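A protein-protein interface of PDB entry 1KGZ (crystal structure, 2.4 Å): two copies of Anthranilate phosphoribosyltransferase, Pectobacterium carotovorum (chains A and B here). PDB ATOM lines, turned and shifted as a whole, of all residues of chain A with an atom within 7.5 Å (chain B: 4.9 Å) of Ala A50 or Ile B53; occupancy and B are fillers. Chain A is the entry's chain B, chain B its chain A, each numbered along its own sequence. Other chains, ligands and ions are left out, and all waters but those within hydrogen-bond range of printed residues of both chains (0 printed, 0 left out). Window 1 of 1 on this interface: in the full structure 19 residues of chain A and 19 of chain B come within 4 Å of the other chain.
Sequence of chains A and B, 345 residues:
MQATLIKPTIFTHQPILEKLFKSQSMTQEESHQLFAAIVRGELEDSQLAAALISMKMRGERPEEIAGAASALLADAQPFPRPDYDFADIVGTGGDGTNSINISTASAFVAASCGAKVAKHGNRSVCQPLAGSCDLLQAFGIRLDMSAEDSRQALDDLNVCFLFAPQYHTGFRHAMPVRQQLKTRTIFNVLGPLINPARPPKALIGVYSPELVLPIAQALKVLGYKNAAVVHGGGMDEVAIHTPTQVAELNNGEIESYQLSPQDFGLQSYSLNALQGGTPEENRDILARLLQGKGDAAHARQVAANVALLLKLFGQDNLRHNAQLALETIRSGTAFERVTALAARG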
ATOM      1  N   LEU A  17       5.231 -21.685  -2.134  1.00  0.00           N
ATOM      2  CA  LEU A  17       6.541 -21.874  -1.523  1.00  0.00           C
ATOM      3  C   LEU A  17       7.567 -22.357  -2.544  1.00  0.00           C
ATOM      4  O   LEU A  17       8.750 -22.029  -2.437  1.00  0.00           O
ATOM      5  CB  LEU A  17       6.463 -22.884  -0.378  1.00  0.00           C
ATOM      6  CG  LEU A  17       5.569 -22.557   0.819  1.00  0.00           C
ATOM      7  CD1 LEU A  17       5.707 -23.665   1.857  1.00  0.00           C
ATOM      8  CD2 LEU A  17       5.968 -21.218   1.424  1.00  0.00           C
ATOM      9  N   LEU A  20       8.668 -19.354  -4.458  1.00  0.00           N
ATOM     10  CA  LEU A  20       9.577 -18.518  -3.666  1.00  0.00           C
ATOM     11  C   LEU A  20      10.997 -19.065  -3.717  1.00  0.00           C
ATOM     12  O   LEU A  20      11.960 -18.300  -3.826  1.00  0.00           O
ATOM     13  CB  LEU A  20       9.123 -18.437  -2.200  1.00  0.00           C
ATOM     14  CG  LEU A  20       8.014 -17.424  -1.878  1.00  0.00           C
ATOM     15  CD1 LEU A  20       7.533 -17.618  -0.460  1.00  0.00           C
ATOM     16  CD2 LEU A  20       8.524 -16.005  -2.087  1.00  0.00           C
ATOM     17  N   PHE A  21      11.121 -20.390  -3.653  1.00  0.00           N
ATOM     18  CA  PHE A  21      12.429 -21.038  -3.674  1.00  0.00           C
ATOM     19  C   PHE A  21      13.129 -20.964  -5.030  1.00  0.00           C
ATOM     20  O   PHE A  21      14.279 -21.398  -5.171  1.00  0.00           O
ATOM     21  CB  PHE A  21      12.307 -22.499  -3.228  1.00  0.00           C
ATOM     22  CG  PHE A  21      11.643 -22.672  -1.885  1.00  0.00           C
ATOM     23  CD1 PHE A  21      11.667 -21.645  -0.936  1.00  0.00           C
ATOM     24  CD2 PHE A  21      10.990 -23.863  -1.566  1.00  0.00           C
ATOM     25  CE1 PHE A  21      11.045 -21.802   0.311  1.00  0.00           C
ATOM     26  CE2 PHE A  21      10.363 -24.034  -0.322  1.00  0.00           C
ATOM     27  CZ  PHE A  21      10.392 -22.999   0.618  1.00  0.00           C
ATOM     28  N   GLU A  44       4.283 -24.713   9.445  1.00  0.00           N
ATOM     29  CA  GLU A  44       5.288 -25.287  10.335  1.00  0.00           C
ATOM     30  C   GLU A  44       6.431 -24.288  10.459  1.00  0.00           C
ATOM     31  O   GLU A  44       6.640 -23.457   9.569  1.00  0.00           O
ATOM     32  CB  GLU A  44       5.847 -26.590   9.747  1.00  0.00           C
ATOM     33  CG  GLU A  44       4.864 -27.738   9.687  1.00  0.00           C
ATOM     34  CD  GLU A  44       4.339 -28.114  11.056  1.00  0.00           C
ATOM     35  OE1 GLU A  44       5.159 -28.269  11.991  1.00  0.00           O
ATOM     36  OE2 GLU A  44       3.107 -28.257  11.198  1.00  0.00           O
ATOM     37  N   ASP A  45       7.173 -24.372  11.556  1.00  0.00           N
ATOM     38  CA  ASP A  45       8.306 -23.475  11.763  1.00  0.00           C
ATOM     39  C   ASP A  45       9.208 -23.483  10.533  1.00  0.00           C
ATOM     40  O   ASP A  45       9.625 -22.432  10.044  1.00  0.00           O
ATOM     41  CB  ASP A  45       9.125 -23.917  12.986  1.00  0.00           C
ATOM     42  CG  ASP A  45       8.506 -23.471  14.302  1.00  0.00           C
ATOM     43  OD1 ASP A  45       7.367 -22.947  14.280  1.00  0.00           O
ATOM     44  OD2 ASP A  45       9.161 -23.647  15.356  1.00  0.00           O
ATOM     45  N   SER A  46       9.496 -24.679  10.032  1.00  0.00           N
ATOM     46  CA  SER A  46      10.369 -24.841   8.879  1.00  0.00           C
ATOM     47  C   SER A  46       9.886 -24.083   7.652  1.00  0.00           C
ATOM     48  O   SER A  46      10.678 -23.424   6.978  1.00  0.00           O
ATOM     49  CB  SER A  46      10.519 -26.332   8.545  1.00  0.00           C
ATOM     50  OG  SER A  46       9.263 -26.929   8.274  1.00  0.00           O
ATOM     51  N   GLN A  47       8.584 -24.166   7.380  1.00  0.00           N
ATOM     52  CA  GLN A  47       7.979 -23.514   6.223  1.00  0.00           C
ATOM     53  C   GLN A  47       7.940 -21.993   6.350  1.00  0.00           C
ATOM     54  O   GLN A  47       8.168 -21.269   5.368  1.00  0.00           O
ATOM     55  CB  GLN A  47       6.550 -24.030   6.018  1.00  0.00           C
ATOM     56  CG  GLN A  47       6.346 -25.485   6.391  1.00  0.00           C
ATOM     57  CD  GLN A  47       4.936 -25.974   6.096  1.00  0.00           C
ATOM     58  OE1 GLN A  47       4.612 -26.321   4.950  1.00  0.00           O
ATOM     59  NE2 GLN A  47       4.085 -25.998   7.125  1.00  0.00           N
ATOM     60  N   LEU A  48       7.635 -21.507   7.547  1.00  0.00           N
ATOM     61  CA  LEU A  48       7.568 -20.069   7.776  1.00  0.00           C
ATOM     62  C   LEU A  48       8.956 -19.486   7.600  1.00  0.00           C
ATOM     63  O   LEU A  48       9.127 -18.466   6.930  1.00  0.00           O
ATOM     64  CB  LEU A  48       7.058 -19.770   9.185  1.00  0.00           C
ATOM     65  CG  LEU A  48       7.051 -18.293   9.606  1.00  0.00           C
ATOM     66  CD1 LEU A  48       6.220 -17.475   8.644  1.00  0.00           C
ATOM     67  CD2 LEU A  48       6.513 -18.178  11.022  1.00  0.00           C
ATOM     68  N   ALA A  49       9.947 -20.138   8.205  1.00  0.00           N
ATOM     69  CA  ALA A  49      11.334 -19.694   8.107  1.00  0.00           C
ATOM     70  C   ALA A  49      11.809 -19.733   6.651  1.00  0.00           C
ATOM     71  O   ALA A  49      12.523 -18.833   6.193  1.00  0.00           O
ATOM     72  CB  ALA A  49      12.224 -20.581   8.968  1.00  0.00           C
ATOM     73  N   ALA A  50      11.406 -20.774   5.924  1.00  0.00           N
ATOM     74  CA  ALA A  50      11.806 -20.912   4.523  1.00  0.00           C
ATOM     75  C   ALA A  50      11.178 -19.782   3.725  1.00  0.00           C
ATOM     76  O   ALA A  50      11.816 -19.175   2.864  1.00  0.00           O
ATOM     77  CB  ALA A  50      11.358 -22.256   3.973  1.00  0.00           C
ATOM     78  N   ALA A  51       9.922 -19.498   4.026  1.00  0.00           N
ATOM     79  CA  ALA A  51       9.216 -18.430   3.346  1.00  0.00           C
ATOM     80  C   ALA A  51       9.885 -17.087   3.627  1.00  0.00           C
ATOM     81  O   ALA A  51      10.124 -16.305   2.707  1.00  0.00           O
ATOM     82  CB  ALA A  51       7.761 -18.397   3.808  1.00  0.00           C
ATOM     83  N   LEU A  52      10.218 -16.829   4.890  1.00  0.00           N
ATOM     84  CA  LEU A  52      10.830 -15.553   5.261  1.00  0.00           C
ATOM     85  C   LEU A  52      12.230 -15.336   4.685  1.00  0.00           C
ATOM     86  O   LEU A  52      12.553 -14.239   4.211  1.00  0.00           O
ATOM     87  CB  LEU A  52      10.860 -15.404   6.787  1.00  0.00           C
ATOM     88  CG  LEU A  52       9.500 -15.377   7.510  1.00  0.00           C
ATOM     89  CD1 LEU A  52       9.693 -15.407   9.032  1.00  0.00           C
ATOM     90  CD2 LEU A  52       8.727 -14.126   7.083  1.00  0.00           C
ATOM     91  N   ILE A  53      13.060 -16.373   4.717  1.00  0.00           N
ATOM     92  CA  ILE A  53      14.420 -16.258   4.194  1.00  0.00           C
ATOM     93  C   ILE A  53      14.453 -16.089   2.673  1.00  0.00           C
ATOM     94  O   ILE A  53      15.241 -15.295   2.143  1.00  0.00           O
ATOM     95  CB  ILE A  53      15.281 -17.496   4.580  1.00  0.00           C
ATOM     96  CG1 ILE A  53      15.364 -17.622   6.100  1.00  0.00           C
ATOM     97  CG2 ILE A  53      16.688 -17.347   4.033  1.00  0.00           C
ATOM     98  CD1 ILE A  53      15.990 -16.402   6.770  1.00  0.00           C
ATOM     99  N   SER A  54      13.596 -16.825   1.972  1.00  0.00           N
ATOM    100  CA  SER A  54      13.563 -16.754   0.513  1.00  0.00           C
ATOM    101  C   SER A  54      13.164 -15.378  -0.012  1.00  0.00           C
ATOM    102  O   SER A  54      13.612 -14.974  -1.073  1.00  0.00           O
ATOM    103  CB  SER A  54      12.620 -17.827  -0.048  1.00  0.00           C
ATOM    104  OG  SER A  54      11.355 -17.773   0.586  1.00  0.00           O
ATOM    105  N   MET A  55      12.312 -14.671   0.724  1.00  0.00           N
ATOM    106  CA  MET A  55      11.872 -13.331   0.331  1.00  0.00           C
ATOM    107  C   MET A  55      12.940 -12.329   0.736  1.00  0.00           C
ATOM    108  O   MET A  55      13.149 -11.310   0.073  1.00  0.00           O
ATOM    109  CB  MET A  55      10.567 -12.960   1.038  1.00  0.00           C
ATOM    110  CG  MET A  55       9.348 -13.752   0.596  1.00  0.00           C
ATOM    111  SD  MET A  55       7.893 -13.227   1.527  1.00  0.00           S
ATOM    112  CE  MET A  55       7.927 -14.398   2.857  1.00  0.00           C
ATOM    113  N   LYS A  56      13.593 -12.624   1.855  1.00  0.00           N
ATOM    114  CA  LYS A  56      14.665 -11.788   2.365  1.00  0.00           C
ATOM    115  C   LYS A  56      15.779 -11.709   1.323  1.00  0.00           C
ATOM    116  O   LYS A  56      16.128 -10.634   0.840  1.00  0.00           O
ATOM    117  CB  LYS A  56      15.217 -12.398   3.659  1.00  0.00           C
ATOM    118  CG  LYS A  56      16.414 -11.659   4.225  1.00  0.00           C
ATOM    119  CD  LYS A  56      16.998 -12.367   5.453  1.00  0.00           C
ATOM    120  CE  LYS A  56      18.240 -11.624   5.978  1.00  0.00           C
ATOM    121  NZ  LYS A  56      17.952 -10.204   6.408  1.00  0.00           N
ATOM    122  N   MET A  57      16.316 -12.869   0.969  1.00  0.00           N
ATOM    123  CA  MET A  57      17.412 -12.974   0.016  1.00  0.00           C
ATOM    124  C   MET A  57      17.166 -12.340  -1.352  1.00  0.00           C
ATOM    125  O   MET A  57      18.062 -11.729  -1.942  1.00  0.00           O
ATOM    126  CB  MET A  57      17.795 -14.450  -0.142  1.00  0.00           C
ATOM    127  CG  MET A  57      18.407 -15.040   1.122  1.00  0.00           C
ATOM    128  SD  MET A  57      18.775 -16.792   0.993  1.00  0.00           S
ATOM    129  CE  MET A  57      20.264 -16.731  -0.076  1.00  0.00           C
ATOM    130  N   VAL A 177       9.876 -18.018  15.615  1.00  0.00           N
ATOM    131  CA  VAL A 177      10.781 -18.117  14.477  1.00  0.00           C
ATOM    132  C   VAL A 177      11.575 -16.831  14.294  1.00  0.00           C
ATOM    133  O   VAL A 177      12.783 -16.873  14.054  1.00  0.00           O
ATOM    134  CB  VAL A 177      10.013 -18.434  13.169  1.00  0.00           C
ATOM    135  CG1 VAL A 177      10.899 -18.168  11.941  1.00  0.00           C
ATOM    136  CG2 VAL A 177       9.580 -19.902  13.171  1.00  0.00           C
ATOM    137  N   LEU A 181      15.679 -16.886  14.232  1.00  0.00           N
ATOM    138  CA  LEU A 181      16.402 -16.473  13.033  1.00  0.00           C
ATOM    139  C   LEU A 181      17.335 -15.278  13.287  1.00  0.00           C
ATOM    140  O   LEU A 181      18.305 -15.084  12.569  1.00  0.00           O
ATOM    141  CB  LEU A 181      15.391 -16.137  11.929  1.00  0.00           C
ATOM    142  CG  LEU A 181      15.220 -17.123  10.764  1.00  0.00           C
ATOM    143  CD1 LEU A 181      15.437 -18.554  11.215  1.00  0.00           C
ATOM    144  CD2 LEU A 181      13.844 -16.937  10.153  1.00  0.00           C
ATOM    145  N   ALA B  49      16.132 -24.928   8.392  1.00  0.00           N
ATOM    146  CA  ALA B  49      15.391 -24.663   7.159  1.00  0.00           C
ATOM    147  C   ALA B  49      15.917 -23.439   6.410  1.00  0.00           C
ATOM    148  O   ALA B  49      15.944 -23.419   5.179  1.00  0.00           O
ATOM    149  CB  ALA B  49      13.921 -24.479   7.471  1.00  0.00           C
ATOM    150  N   ALA B  50      16.322 -22.417   7.155  1.00  0.00           N
ATOM    151  CA  ALA B  50      16.848 -21.201   6.555  1.00  0.00           C
ATOM    152  C   ALA B  50      18.192 -21.532   5.906  1.00  0.00           C
ATOM    153  O   ALA B  50      18.528 -21.016   4.835  1.00  0.00           O
ATOM    154  CB  ALA B  50      17.023 -20.127   7.623  1.00  0.00           C
ATOM    155  N   ALA B  51      18.957 -22.396   6.567  1.00  0.00           N
ATOM    156  CA  ALA B  51      20.251 -22.822   6.046  1.00  0.00           C
ATOM    157  C   ALA B  51      20.040 -23.579   4.733  1.00  0.00           C
ATOM    158  O   ALA B  51      20.612 -23.226   3.705  1.00  0.00           O
ATOM    159  CB  ALA B  51      20.960 -23.727   7.063  1.00  0.00           C
ATOM    160  N   LEU B  52      19.201 -24.612   4.775  1.00  0.00           N
ATOM    161  CA  LEU B  52      18.921 -25.436   3.600  1.00  0.00           C
ATOM    162  C   LEU B  52      18.352 -24.654   2.415  1.00  0.00           C
ATOM    163  O   LEU B  52      18.709 -24.916   1.265  1.00  0.00           O
ATOM    164  CB  LEU B  52      17.954 -26.565   3.979  1.00  0.00           C
ATOM    165  CG  LEU B  52      18.536 -27.859   4.572  1.00  0.00           C
ATOM    166  CD1 LEU B  52      19.673 -27.537   5.523  1.00  0.00           C
ATOM    167  CD2 LEU B  52      17.427 -28.647   5.280  1.00  0.00           C
ATOM    168  N   ILE B  53      17.476 -23.692   2.699  1.00  0.00           N
ATOM    169  CA  ILE B  53      16.851 -22.891   1.650  1.00  0.00           C
ATOM    170  C   ILE B  53      17.780 -21.816   1.085  1.00  0.00           C
ATOM    171  O   ILE B  53      17.771 -21.561  -0.114  1.00  0.00           O
ATOM    172  CB  ILE B  53      15.551 -22.230   2.173  1.00  0.00           C
ATOM    173  CG1 ILE B  53      14.522 -23.320   2.478  1.00  0.00           C
ATOM    174  CG2 ILE B  53      14.986 -21.256   1.149  1.00  0.00           C
ATOM    175  CD1 ILE B  53      14.078 -24.096   1.251  1.00  0.00           C
ATOM    176  N   SER B  54      18.569 -21.178   1.944  1.00  0.00           N
ATOM    177  CA  SER B  54      19.493 -20.150   1.482  1.00  0.00           C
ATOM    178  C   SER B  54      20.561 -20.766   0.573  1.00  0.00           C
ATOM    179  O   SER B  54      20.988 -20.145  -0.405  1.00  0.00           O
ATOM    180  CB  SER B  54      20.156 -19.457   2.673  1.00  0.00           C
ATOM    181  OG  SER B  54      20.609 -20.407   3.625  1.00  0.00           O
ATOM    182  N   MET B  55      20.990 -21.986   0.902  1.00  0.00           N
ATOM    183  CA  MET B  55      21.996 -22.668   0.103  1.00  0.00           C
ATOM    184  C   MET B  55      21.368 -23.062  -1.222  1.00  0.00           C
ATOM    185  O   MET B  55      21.983 -22.927  -2.279  1.00  0.00           O
ATOM    186  CB  MET B  55      22.495 -23.929   0.813  1.00  0.00           C
ATOM    187  CG  MET B  55      23.296 -23.678   2.084  1.00  0.00           C
ATOM    188  SD  MET B  55      24.006 -25.198   2.756  1.00  0.00           S
ATOM    189  CE  MET B  55      22.633 -25.849   3.681  1.00  0.00           C
ATOM    190  N   LYS B  56      20.137 -23.560  -1.140  1.00  0.00           N
ATOM    191  CA  LYS B  56      19.372 -24.003  -2.296  1.00  0.00           C
ATOM    192  C   LYS B  56      19.214 -22.911  -3.340  1.00  0.00           C
ATOM    193  O   LYS B  56      19.615 -23.078  -4.494  1.00  0.00           O
ATOM    194  CB  LYS B  56      17.982 -24.474  -1.847  1.00  0.00           C
ATOM    195  CG  LYS B  56      17.040 -24.865  -2.986  1.00  0.00           C
ATOM    196  CD  LYS B  56      15.641 -25.170  -2.457  1.00  0.00           C
ATOM    197  CE  LYS B  56      14.657 -25.419  -3.585  1.00  0.00           C
ATOM    198  NZ  LYS B  56      14.978 -26.651  -4.353  1.00  0.00           N
ATOM    199  N   MET B  57      18.615 -21.795  -2.932  1.00  0.00           N
ATOM    200  CA  MET B  57      18.387 -20.682  -3.833  1.00  0.00           C
ATOM    201  C   MET B  57      19.649 -20.153  -4.508  1.00  0.00           C
ATOM    202  O   MET B  57      19.615 -19.759  -5.677  1.00  0.00           O
ATOM    203  CB  MET B  57      17.689 -19.555  -3.089  1.00  0.00           C
ATOM    204  CG  MET B  57      16.233 -19.839  -2.785  1.00  0.00           C
ATOM    205  SD  MET B  57      15.520 -18.455  -1.897  1.00  0.00           S
ATOM    206  CE  MET B  57      15.656 -17.159  -3.148  1.00  0.00           C
ATOM    207  N   LEU B 181       9.270 -29.626   4.366  1.00  0.00           N
ATOM    208  CA  LEU B 181       9.711 -28.702   3.329  1.00  0.00           C
ATOM    209  C   LEU B 181       9.329 -29.192   1.926  1.00  0.00           C
ATOM    210  O   LEU B 181       9.219 -28.397   0.984  1.00  0.00           O
ATOM    211  CB  LEU B 181      11.225 -28.511   3.452  1.00  0.00           C
ATOM    212  CG  LEU B 181      11.801 -27.091   3.489  1.00  0.00           C
ATOM    213  CD1 LEU B 181      10.975 -26.179   4.397  1.00  0.00           C
ATOM    214  CD2 LEU B 181      13.229 -27.168   3.974  1.00  0.00           C
ATOM    215  N   THR B 183      10.680 -30.202  -0.602  1.00  0.00           N
ATOM    216  CA  THR B 183      11.407 -29.626  -1.725  1.00  0.00           C
ATOM    217  C   THR B 183      12.828 -30.165  -1.681  1.00  0.00           C
ATOM    218  O   THR B 183      13.322 -30.545  -0.616  1.00  0.00           O
ATOM    219  CB  THR B 183      11.463 -28.082  -1.659  1.00  0.00           C
ATOM    220  OG1 THR B 183      11.928 -27.566  -2.914  1.00  0.00           O
ATOM    221  CG2 THR B 183      12.421 -27.620  -0.563  1.00  0.00           C
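OG of Ser B54 lies within hydrogen-bond range of O of Ala B50 (2.5 Å).
The backbone carbonyl oxygen (O) of Ala B51 lies within hydrogen-bond range of the side-chain hydroxyl (OG) of Ser B54 (2.8 Å).
The side-chain amino group (NZ) of Lys B56 lies within hydrogen-bond range of the side-chain hydroxyl (OG1) of Thr B183 (3.5 Å).
The backbone carbonyl oxygen (O) of Ala A50 is in hydrogen-bond range of the side-chain hydroxyl (OG) of Ser A54 (2.7 Å).
The backbone carbonyl oxygen (O) of Ala A51 is in hydrogen-bond range of the side-chain hydroxyl (OG) of Ser A54.
Among the printed residues, merely in contact across the chains: Ile A53 with Ala B50, Met A57 with Ser B54, Ser A46 with Ala B49, Phe A21 with Met B57, Ser A54 with Met B57, Ala A50 with Ile B53, Phe A21 with Lys B56, Ser A46 with Leu B181, Phe A21 with Ile B53, Leu A20 with Met B57 and Ala A50 with Leu B181.
Of the printed residues of chain B, Phe A21 touches Ile B53 (3.9 Å), Lys B56 (3.8 Å) and Met B57 (3.5 Å).
Of the printed residues of chain B, Ser A54 touches Met B57 (3.5 Å).
Ile B53 touches just these residues of chain A: Phe A21 (3.9 Å) and Ala A50 (3.7 Å).
Thr B183 touches none of the printed residues of chain A.
The nearest residue of chain B that does not touch Ala A50 is Ala B49 (4.7 Å).
The nearest residue of chain A that does not touch Ile B53 is Ser A54 (4.3 Å).
Of the 11 printed residues of chain B, 7 touch a printed residue of chain A.
Printed residues of chain B that touch a printed residue of chain A: Ala B49, Ala B50, Ile B53, Ser B54, Lys B56, Met B57 and Leu B181.
Hydrophobic or aromatic side chains of chain B within 4 Å of the printed part of chain A: Ala B49, Ala B50, Ile B53, Met B57 and Leu B181.
Along chain B the printed residues that touch a printed residue of chain A span positions 49 to 181.
Of the 19 printed residues of chain A, 7 touch a printed residue of chain B.
Along chain A the printed residues that touch a printed residue of chain B span positions 20 to 57.
Among the printed residues, no Asp or Glu carboxylate lies within 4 Å of a Lys or Arg side-chain nitrogen of the other chain.
Ala A50 touches Ile B53, and with the chains exchanged Ile A53 touches Ala B50.
Ala A50 touches Leu B181, but with the chains exchanged Leu A181 does not touch Ala B50 (4.2 Å).
Ser A54 touches Met B57, and with the chains exchanged Met A57 touches Ser B54.
Of the 11 pairs that touch across the chains among the printed residues, 4 have their exchanged pair printed and touching as well.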
